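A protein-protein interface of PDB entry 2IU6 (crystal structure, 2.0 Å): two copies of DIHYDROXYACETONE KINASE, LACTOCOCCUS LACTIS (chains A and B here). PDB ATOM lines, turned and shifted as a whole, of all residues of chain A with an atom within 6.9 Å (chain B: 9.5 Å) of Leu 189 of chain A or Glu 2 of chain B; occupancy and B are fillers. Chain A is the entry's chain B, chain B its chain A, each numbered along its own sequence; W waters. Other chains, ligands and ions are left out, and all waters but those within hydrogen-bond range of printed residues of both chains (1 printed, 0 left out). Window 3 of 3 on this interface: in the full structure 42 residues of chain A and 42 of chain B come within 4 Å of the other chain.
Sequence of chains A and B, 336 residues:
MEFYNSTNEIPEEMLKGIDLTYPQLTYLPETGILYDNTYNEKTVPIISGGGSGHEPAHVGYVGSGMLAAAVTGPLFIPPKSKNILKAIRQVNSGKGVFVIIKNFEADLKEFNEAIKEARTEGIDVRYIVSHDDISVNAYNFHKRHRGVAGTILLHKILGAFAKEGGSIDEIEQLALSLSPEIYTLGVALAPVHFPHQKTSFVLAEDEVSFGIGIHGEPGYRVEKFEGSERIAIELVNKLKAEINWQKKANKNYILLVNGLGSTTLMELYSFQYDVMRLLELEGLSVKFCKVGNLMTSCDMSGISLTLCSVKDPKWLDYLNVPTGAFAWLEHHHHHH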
ATOM      1  N   VAL A 187      -8.359  -7.459  11.518  1.00  0.00           N
ATOM      2  CA  VAL A 187      -9.490  -8.386  11.376  1.00  0.00           C
ATOM      3  C   VAL A 187     -10.605  -7.828  12.245  1.00  0.00           C
ATOM      4  O   VAL A 187     -10.318  -7.243  13.294  1.00  0.00           O
ATOM      5  CB  VAL A 187      -9.075  -9.826  11.874  1.00  0.00           C
ATOM      6  CG1 VAL A 187      -8.568  -9.823  13.330  1.00  0.00           C
ATOM      7  CG2 VAL A 187     -10.228 -10.842  11.682  1.00  0.00           C
ATOM      8  N   ALA A 188     -11.873  -7.993  11.857  1.00  0.00           N
ATOM      9  CA  ALA A 188     -12.942  -7.548  12.752  1.00  0.00           C
ATOM     10  C   ALA A 188     -13.947  -8.669  12.933  1.00  0.00           C
ATOM     11  O   ALA A 188     -14.070  -9.537  12.062  1.00  0.00           O
ATOM     12  CB  ALA A 188     -13.631  -6.298  12.189  1.00  0.00           C
ATOM     13  N   LEU A 189     -14.661  -8.656  14.056  1.00  0.00           N
ATOM     14  CA  LEU A 189     -15.810  -9.562  14.239  1.00  0.00           C
ATOM     15  C   LEU A 189     -17.099  -8.777  14.120  1.00  0.00           C
ATOM     16  O   LEU A 189     -17.171  -7.646  14.585  1.00  0.00           O
ATOM     17  CB  LEU A 189     -15.798 -10.211  15.630  1.00  0.00           C
ATOM     18  CG  LEU A 189     -14.537 -10.991  16.041  1.00  0.00           C
ATOM     19  CD1 LEU A 189     -14.870 -11.767  17.333  1.00  0.00           C
ATOM     20  CD2 LEU A 189     -14.222 -11.991  14.943  1.00  0.00           C
ATOM     21  N   ALA A 190     -18.115  -9.375  13.503  1.00  0.00           N
ATOM     22  CA  ALA A 190     -19.460  -8.824  13.566  1.00  0.00           C
ATOM     23  C   ALA A 190     -20.551  -9.903  13.678  1.00  0.00           C
ATOM     24  O   ALA A 190     -20.434 -11.001  13.122  1.00  0.00           O
ATOM     25  CB  ALA A 190     -19.718  -7.905  12.382  1.00  0.00           C
ATOM     26  N   PRO A 191     -21.629  -9.586  14.411  1.00  0.00           N
ATOM     27  CA  PRO A 191     -22.754 -10.527  14.610  1.00  0.00           C
ATOM     28  C   PRO A 191     -23.521 -10.813  13.322  1.00  0.00           C
ATOM     29  O   PRO A 191     -23.694  -9.927  12.491  1.00  0.00           O
ATOM     30  CB  PRO A 191     -23.667  -9.786  15.593  1.00  0.00           C
ATOM     31  CG  PRO A 191     -22.787  -8.719  16.220  1.00  0.00           C
ATOM     32  CD  PRO A 191     -21.849  -8.308  15.106  1.00  0.00           C
ATOM     33  N   ASP A 206     -18.644 -13.589  15.234  1.00  0.00           N
ATOM     34  CA  ASP A 206     -19.628 -14.442  14.514  1.00  0.00           C
ATOM     35  C   ASP A 206     -19.386 -14.610  13.013  1.00  0.00           C
ATOM     36  O   ASP A 206     -19.211 -15.748  12.576  1.00  0.00           O
ATOM     37  CB  ASP A 206     -21.034 -13.978  14.794  1.00  0.00           C
ATOM     38  CG  ASP A 206     -22.037 -15.074  14.572  1.00  0.00           C
ATOM     39  OD1 ASP A 206     -23.241 -14.812  14.786  1.00  0.00           O
ATOM     40  OD2 ASP A 206     -21.596 -16.180  14.177  1.00  0.00           O
ATOM     41  N   GLU A 207     -19.371 -13.520  12.234  1.00  0.00           N
ATOM     42  CA  GLU A 207     -18.517 -13.459  11.036  1.00  0.00           C
ATOM     43  C   GLU A 207     -17.201 -12.689  11.266  1.00  0.00           C
ATOM     44  O   GLU A 207     -17.131 -11.749  12.054  1.00  0.00           O
ATOM     45  CB  GLU A 207     -19.225 -12.932   9.783  1.00  0.00           C
ATOM     46  CG  GLU A 207     -19.717 -11.489   9.861  1.00  0.00           C
ATOM     47  CD  GLU A 207     -20.096 -10.842   8.506  1.00  0.00           C
ATOM     48  OE1 GLU A 207     -20.537 -11.554   7.559  1.00  0.00           O
ATOM     49  OE2 GLU A 207     -19.940  -9.590   8.410  1.00  0.00           O
ATOM     50  N   VAL A 208     -16.172 -13.110  10.556  1.00  0.00           N
ATOM     51  CA  VAL A 208     -14.824 -12.620  10.767  1.00  0.00           C
ATOM     52  C   VAL A 208     -14.481 -11.998   9.423  1.00  0.00           C
ATOM     53  O   VAL A 208     -14.588 -12.676   8.402  1.00  0.00           O
ATOM     54  CB  VAL A 208     -13.880 -13.829  11.078  1.00  0.00           C
ATOM     55  CG1 VAL A 208     -12.417 -13.416  11.132  1.00  0.00           C
ATOM     56  CG2 VAL A 208     -14.239 -14.464  12.402  1.00  0.00           C
ATOM     57  N   SER A 209     -14.081 -10.724   9.416  1.00  0.00           N
ATOM     58  CA  SER A 209     -13.581 -10.076   8.200  1.00  0.00           C
ATOM     59  C   SER A 209     -12.080  -9.825   8.332  1.00  0.00           C
ATOM     60  O   SER A 209     -11.671  -8.985   9.156  1.00  0.00           O
ATOM     61  CB  SER A 209     -14.250  -8.727   7.983  1.00  0.00           C
ATOM     62  OG  SER A 209     -15.653  -8.898   7.864  1.00  0.00           O
ATOM     63  N   PHE A 225     -16.884 -17.468  12.326  1.00  0.00           N
ATOM     64  CA  PHE A 225     -15.934 -17.590  13.439  1.00  0.00           C
ATOM     65  C   PHE A 225     -15.848 -19.049  13.907  1.00  0.00           C
ATOM     66  O   PHE A 225     -16.857 -19.656  14.236  1.00  0.00           O
ATOM     67  CB  PHE A 225     -16.339 -16.643  14.570  1.00  0.00           C
ATOM     68  CG  PHE A 225     -15.458 -16.722  15.790  1.00  0.00           C
ATOM     69  CD1 PHE A 225     -14.220 -16.086  15.825  1.00  0.00           C
ATOM     70  CD2 PHE A 225     -15.888 -17.439  16.914  1.00  0.00           C
ATOM     71  CE1 PHE A 225     -13.411 -16.156  16.950  1.00  0.00           C
ATOM     72  CE2 PHE A 225     -15.088 -17.517  18.048  1.00  0.00           C
ATOM     73  CZ  PHE A 225     -13.846 -16.875  18.064  1.00  0.00           C
ATOM     74  N   SER A 228     -10.004 -18.322  17.448  1.00  0.00           N
ATOM     75  CA  SER A 228      -9.016 -17.310  17.130  1.00  0.00           C
ATOM     76  C   SER A 228      -7.661 -17.835  16.708  1.00  0.00           C
ATOM     77  O   SER A 228      -6.902 -17.117  16.093  1.00  0.00           O
ATOM     78  CB  SER A 228      -8.879 -16.406  18.330  1.00  0.00           C
ATOM     79  OG  SER A 228     -10.011 -15.553  18.342  1.00  0.00           O
ATOM     80  N   ILE A 231      -7.755 -17.449  13.080  1.00  0.00           N
ATOM     81  CA  ILE A 231      -7.605 -16.040  12.768  1.00  0.00           C
ATOM     82  C   ILE A 231      -6.119 -15.636  12.815  1.00  0.00           C
ATOM     83  O   ILE A 231      -5.596 -14.942  11.918  1.00  0.00           O
ATOM     84  CB  ILE A 231      -8.463 -15.197  13.698  1.00  0.00           C
ATOM     85  CG1 ILE A 231      -9.953 -15.571  13.512  1.00  0.00           C
ATOM     86  CG2 ILE A 231      -8.226 -13.717  13.394  1.00  0.00           C
ATOM     87  CD1 ILE A 231     -10.901 -14.781  14.441  1.00  0.00           C
ATOM     88  N   THR A 263     -12.673  -4.793  21.725  1.00  0.00           N
ATOM     89  CA  THR A 263     -12.069  -6.081  22.119  1.00  0.00           C
ATOM     90  C   THR A 263     -11.436  -5.966  23.510  1.00  0.00           C
ATOM     91  O   THR A 263     -10.793  -4.970  23.814  1.00  0.00           O
ATOM     92  CB  THR A 263     -10.954  -6.412  21.106  1.00  0.00           C
ATOM     93  OG1 THR A 263     -11.572  -6.472  19.817  1.00  0.00           O
ATOM     94  CG2 THR A 263     -10.225  -7.753  21.424  1.00  0.00           C
ATOM     95  N   THR A 264     -11.624  -6.973  24.349  1.00  0.00           N
ATOM     96  CA  THR A 264     -11.202  -6.891  25.754  1.00  0.00           C
ATOM     97  C   THR A 264      -9.702  -7.168  25.900  1.00  0.00           C
ATOM     98  O   THR A 264      -9.093  -7.732  24.999  1.00  0.00           O
ATOM     99  CB  THR A 264     -11.983  -7.882  26.600  1.00  0.00           C
ATOM    100  OG1 THR A 264     -11.688  -9.220  26.180  1.00  0.00           O
ATOM    101  CG2 THR A 264     -13.490  -7.659  26.385  1.00  0.00           C
ATOM    102  N   MET A 266      -8.528  -9.298  27.868  1.00  0.00           N
ATOM    103  CA  MET A 266      -8.373 -10.740  27.881  1.00  0.00           C
ATOM    104  C   MET A 266      -8.176 -11.245  26.447  1.00  0.00           C
ATOM    105  O   MET A 266      -7.322 -12.106  26.185  1.00  0.00           O
ATOM    106  CB  MET A 266      -9.608 -11.391  28.498  1.00  0.00           C
ATOM    107  CG  MET A 266      -9.517 -12.894  28.682  1.00  0.00           C
ATOM    108  SD  MET A 266      -9.943 -13.851  27.204  1.00  0.00           S
ATOM    109  CE  MET A 266     -11.717 -13.616  27.132  1.00  0.00           C
ATOM    110  N   GLU A 267      -8.960 -10.739  25.501  1.00  0.00           N
ATOM    111  CA  GLU A 267      -8.881 -11.251  24.128  1.00  0.00           C
ATOM    112  C   GLU A 267      -7.576 -10.810  23.490  1.00  0.00           C
ATOM    113  O   GLU A 267      -6.963 -11.544  22.725  1.00  0.00           O
ATOM    114  CB  GLU A 267     -10.026 -10.679  23.291  1.00  0.00           C
ATOM    115  CG  GLU A 267     -11.381 -11.292  23.640  1.00  0.00           C
ATOM    116  CD  GLU A 267     -12.500 -10.430  23.068  1.00  0.00           C
ATOM    117  OE1 GLU A 267     -12.890  -9.440  23.717  1.00  0.00           O
ATOM    118  OE2 GLU A 267     -12.996 -10.734  21.966  1.00  0.00           O
ATOM    119  N   MET A 300     -15.072  -0.468  17.262  1.00  0.00           N
ATOM    120  CA  MET A 300     -14.990  -1.669  16.441  1.00  0.00           C
ATOM    121  C   MET A 300     -14.494  -2.862  17.263  1.00  0.00           C
ATOM    122  O   MET A 300     -13.564  -2.732  18.078  1.00  0.00           O
ATOM    123  CB  MET A 300     -13.936  -1.427  15.344  1.00  0.00           C
ATOM    124  CG  MET A 300     -13.728  -2.659  14.454  1.00  0.00           C
ATOM    125  SD  MET A 300     -12.638  -2.307  13.050  1.00  0.00           S
ATOM    126  CE  MET A 300     -13.603  -1.180  12.019  1.00  0.00           C
ATOM    127  N   SER A 301     -15.083  -4.027  17.062  1.00  0.00           N
ATOM    128  CA  SER A 301     -14.556  -5.257  17.638  1.00  0.00           C
ATOM    129  C   SER A 301     -13.517  -5.840  16.688  1.00  0.00           C
ATOM    130  O   SER A 301     -13.868  -6.521  15.727  1.00  0.00           O
ATOM    131  CB  SER A 301     -15.680  -6.282  17.799  1.00  0.00           C
ATOM    132  OG  SER A 301     -16.426  -5.986  18.970  1.00  0.00           O
ATOM    133  N   GLY A 302     -12.237  -5.607  16.933  1.00  0.00           N
ATOM    134  CA  GLY A 302     -11.263  -6.224  16.064  1.00  0.00           C
ATOM    135  C   GLY A 302      -9.889  -6.051  16.640  1.00  0.00           C
ATOM    136  O   GLY A 302      -9.784  -5.419  17.699  1.00  0.00           O
ATOM    137  N   ILE A 303      -8.883  -6.606  15.951  1.00  0.00           N
ATOM    138  CA  ILE A 303      -7.458  -6.484  16.326  1.00  0.00           C
ATOM    139  C   ILE A 303      -6.629  -6.171  15.098  1.00  0.00           C
ATOM    140  O   ILE A 303      -6.927  -6.667  14.013  1.00  0.00           O
ATOM    141  CB  ILE A 303      -6.969  -7.848  16.949  1.00  0.00           C
ATOM    142  CG1 ILE A 303      -7.887  -8.203  18.121  1.00  0.00           C
ATOM    143  CG2 ILE A 303      -5.488  -7.864  17.308  1.00  0.00           C
ATOM    144  CD1 ILE A 303      -7.694  -9.643  18.677  1.00  0.00           C
ATOM    145  N   GLU B   2     -16.728 -12.014  20.369  1.00  0.00           N
ATOM    146  CA  GLU B   2     -15.527 -12.239  21.251  1.00  0.00           C
ATOM    147  C   GLU B   2     -14.558 -13.283  20.649  1.00  0.00           C
ATOM    148  O   GLU B   2     -14.986 -14.358  20.227  1.00  0.00           O
ATOM    149  CB  GLU B   2     -15.983 -12.669  22.658  1.00  0.00           C
ATOM    150  CG  GLU B   2     -16.622 -14.064  22.657  1.00  0.00           C
ATOM    151  CD  GLU B   2     -17.469 -14.362  23.893  1.00  0.00           C
ATOM    152  OE1 GLU B   2     -18.148 -15.420  23.904  1.00  0.00           O
ATOM    153  OE2 GLU B   2     -17.456 -13.551  24.847  1.00  0.00           O
ATOM    154  N   PHE B   3     -13.259 -12.954  20.623  1.00  0.00           N
ATOM    155  CA  PHE B   3     -12.193 -13.798  20.055  1.00  0.00           C
ATOM    156  C   PHE B   3     -11.851 -15.007  20.955  1.00  0.00           C
ATOM    157  O   PHE B   3     -11.371 -16.024  20.492  1.00  0.00           O
ATOM    158  CB  PHE B   3     -10.930 -12.938  19.825  1.00  0.00           C
ATOM    159  CG  PHE B   3     -11.073 -11.907  18.723  1.00  0.00           C
ATOM    160  CD1 PHE B   3     -10.845 -12.243  17.390  1.00  0.00           C
ATOM    161  CD2 PHE B   3     -11.431 -10.601  19.018  1.00  0.00           C
ATOM    162  CE1 PHE B   3     -10.980 -11.278  16.364  1.00  0.00           C
ATOM    163  CE2 PHE B   3     -11.569  -9.637  18.008  1.00  0.00           C
ATOM    164  CZ  PHE B   3     -11.345  -9.962  16.689  1.00  0.00           C
ATOM    165  N   TYR B   4     -12.103 -14.877  22.255  1.00  0.00           N
ATOM    166  CA  TYR B   4     -11.804 -15.923  23.237  1.00  0.00           C
ATOM    167  C   TYR B   4     -12.890 -15.842  24.312  1.00  0.00           C
ATOM    168  O   TYR B   4     -13.482 -14.778  24.544  1.00  0.00           O
ATOM    169  CB  TYR B   4     -10.439 -15.669  23.896  1.00  0.00           C
ATOM    170  CG  TYR B   4      -9.302 -15.779  22.923  1.00  0.00           C
ATOM    171  CD1 TYR B   4      -8.634 -16.995  22.754  1.00  0.00           C
ATOM    172  CD2 TYR B   4      -8.894 -14.670  22.160  1.00  0.00           C
ATOM    173  CE1 TYR B   4      -7.576 -17.117  21.850  1.00  0.00           C
ATOM    174  CE2 TYR B   4      -7.830 -14.782  21.247  1.00  0.00           C
ATOM    175  CZ  TYR B   4      -7.178 -16.005  21.101  1.00  0.00           C
ATOM    176  OH  TYR B   4      -6.132 -16.159  20.215  1.00  0.00           O
ATOM    177  N   ASN B   5     -13.137 -16.971  24.961  1.00  0.00           N
ATOM    178  CA  ASN B   5     -14.149 -17.046  26.002  1.00  0.00           C
ATOM    179  C   ASN B   5     -13.608 -17.890  27.156  1.00  0.00           C
ATOM    180  O   ASN B   5     -13.317 -19.074  26.964  1.00  0.00           O
ATOM    181  CB  ASN B   5     -15.402 -17.735  25.443  1.00  0.00           C
ATOM    182  CG  ASN B   5     -16.264 -18.347  26.539  1.00  0.00           C
ATOM    183  OD1 ASN B   5     -16.502 -19.573  26.572  1.00  0.00           O
ATOM    184  ND2 ASN B   5     -16.736 -17.495  27.443  1.00  0.00           N
ATOM    185  N   SER B   6     -13.476 -17.299  28.343  1.00  0.00           N
ATOM    186  CA  SER B   6     -12.859 -18.010  29.464  1.00  0.00           C
ATOM    187  C   SER B   6     -13.851 -18.430  30.560  1.00  0.00           C
ATOM    188  O   SER B   6     -13.494 -18.550  31.735  1.00  0.00           O
ATOM    189  CB  SER B   6     -11.709 -17.197  30.055  1.00  0.00           C
ATOM    190  OG  SER B   6     -12.224 -16.090  30.767  1.00  0.00           O
ATOM    191  N   THR B   7     -15.096 -18.650  30.155  1.00  0.00           N
ATOM    192  CA  THR B   7     -16.074 -19.328  30.997  1.00  0.00           C
ATOM    193  C   THR B   7     -15.529 -20.649  31.554  1.00  0.00           C
ATOM    194  O   THR B   7     -15.183 -21.580  30.816  1.00  0.00           O
ATOM    195  CB  THR B   7     -17.411 -19.549  30.240  1.00  0.00           C
ATOM    196  OG1 THR B   7     -17.901 -18.294  29.748  1.00  0.00           O
ATOM    197  CG2 THR B   7     -18.460 -20.180  31.141  1.00  0.00           C
ATOM    198  N   LEU B  75     -13.799 -16.689  34.136  1.00  0.00           N
ATOM    199  CA  LEU B  75     -14.704 -15.534  33.981  1.00  0.00           C
ATOM    200  C   LEU B  75     -15.680 -15.368  35.170  1.00  0.00           C
ATOM    201  O   LEU B  75     -16.461 -16.258  35.447  1.00  0.00           O
ATOM    202  CB  LEU B  75     -15.506 -15.715  32.687  1.00  0.00           C
ATOM    203  CG  LEU B  75     -16.596 -14.679  32.407  1.00  0.00           C
ATOM    204  CD1 LEU B  75     -16.006 -13.301  32.319  1.00  0.00           C
ATOM    205  CD2 LEU B  75     -17.303 -15.033  31.102  1.00  0.00           C
ATOM    206  N   CYS B 298     -16.345  -7.303  31.169  1.00  0.00           N
ATOM    207  CA  CYS B 298     -16.385  -7.745  29.781  1.00  0.00           C
ATOM    208  C   CYS B 298     -16.372  -6.609  28.777  1.00  0.00           C
ATOM    209  O   CYS B 298     -15.490  -5.785  28.839  1.00  0.00           O
ATOM    210  CB  CYS B 298     -17.534  -8.739  29.532  1.00  0.00           C
ATOM    211  SG  CYS B 298     -17.122 -10.277  30.338  1.00  0.00           S
ATOM    212  N   ASP B 299     -17.333  -6.560  27.862  1.00  0.00           N
ATOM    213  CA  ASP B 299     -17.408  -5.435  26.931  1.00  0.00           C
ATOM    214  C   ASP B 299     -18.556  -4.446  27.211  1.00  0.00           C
ATOM    215  O   ASP B 299     -19.110  -3.840  26.292  1.00  0.00           O
ATOM    216  CB  ASP B 299     -17.516  -5.985  25.514  1.00  0.00           C
ATOM    217  CG  ASP B 299     -18.752  -6.855  25.309  1.00  0.00           C
ATOM    218  OD1 ASP B 299     -19.409  -7.287  26.292  1.00  0.00           O
ATOM    219  OD2 ASP B 299     -19.065  -7.108  24.123  1.00  0.00           O
HETATM  220  O   HOH W   1     -10.799 -18.687  20.257  1.00  0.00           O
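The side-chain hydroxyl (OG) of Ser 228 of chain A is in hydrogen-bond range of the backbone carbonyl oxygen (O) of Phe 3 of chain B (2.6 Å). N of Phe 3 of chain B sits at hydrogen-bond distance from OE2 of Glu 267 of chain A.
The backbone carbonyl oxygen (O) of Ile 303 of chain A sits at hydrogen-bond distance from the backbone NH (N) of Val 187 of chain A, at 3.0 Å. The backbone NH (N) of Leu 189 of chain A lies within hydrogen-bond range of the backbone carbonyl oxygen (O) of Ser 301 of chain A, at 2.8 Å. The side-chain carboxylate (OE1) of Glu 267 of chain A sits at hydrogen-bond distance from the side-chain hydroxyl (OG1) of Thr 264 of chain A (2.7 Å). The side-chain hydroxyl (OG1) of Thr 263 of chain A sits at hydrogen-bond distance from the backbone carbonyl oxygen (O) of Gly 302 of chain A, 3.0 Å away. The backbone carbonyl oxygen (O) of Asp 206 of chain A lies within hydrogen-bond range of the backbone NH (N) of Phe 225 of chain A.
Leu 189 of chain A touches Glu 2 of chain B. Phe 3 of chain B touches Leu 189 of chain A (CZ to CG, 3.4 Å). CB of Ser 228 of chain A touches CZ of Tyr 4 of chain B, 3.3 Å away. Phe 3 of chain B touches Ile 231 of chain A. Thr 263 of chain A touches Phe 3 of chain B. Thr 264 of chain A touches Cys 298 of chain B (CG2 to O, 3.7 Å). Tyr 4 of chain B touches Met 266 of chain A. Glu 2 of chain B touches Glu 267 of chain A. Tyr 4 of chain B touches Glu 267 of chain A. CZ of Phe 3 of chain B touches CA of Gly 302 of chain A, 3.8 Å away.
Leu 189 of chain A touches two residues of chain B. Glu 2 of chain B touches three residues of chain A. No residue of chain B comes within 4 Å of Ala 188 of chain A. No residue of chain B comes within 4 Å of Ala 190 of chain A. Printed residues of chain B within 4 Å of Ile 231 of chain A: Phe 3. Of the printed residues of chain B, Met 266 of chain A touches Tyr 4. Printed residues of chain B within 4 Å of Thr 264 of chain A: Cys 298. The nearest residue of chain B that does not touch Leu 189 of chain A is Tyr 4 of chain B (6.4 Å). The nearest printed residue of chain B that does not touch Gly 302 of chain A is Glu 2 of chain B (8.5 Å).
Hydrophobic or aromatic side chains of chain B that line the printed part of chain A: Phe 3 and Tyr 4. Printed residues of chain A that touch a printed residue of chain B: Leu 189, Phe 225, Ser 228, Ile 231, Thr 263, Thr 264, Met 266, Glu 267, Gly 302 and Ile 303. Hydrophobic or aromatic side chains of chain A that line the printed part of chain B: Leu 189, Phe 225, Ile 231, Met 266 and Ile 303. Among the printed residues, 15 pairs touch across the chains.
No position is printed for both chains. Of the 15 pairs that touch across the chains among the printed residues, none has its exchanged pair printed and touching as well.
Water W1 bridges O of Phe 3 of chain B (2.7 Å) and N of Ser 228 of chain A (2.9 Å).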
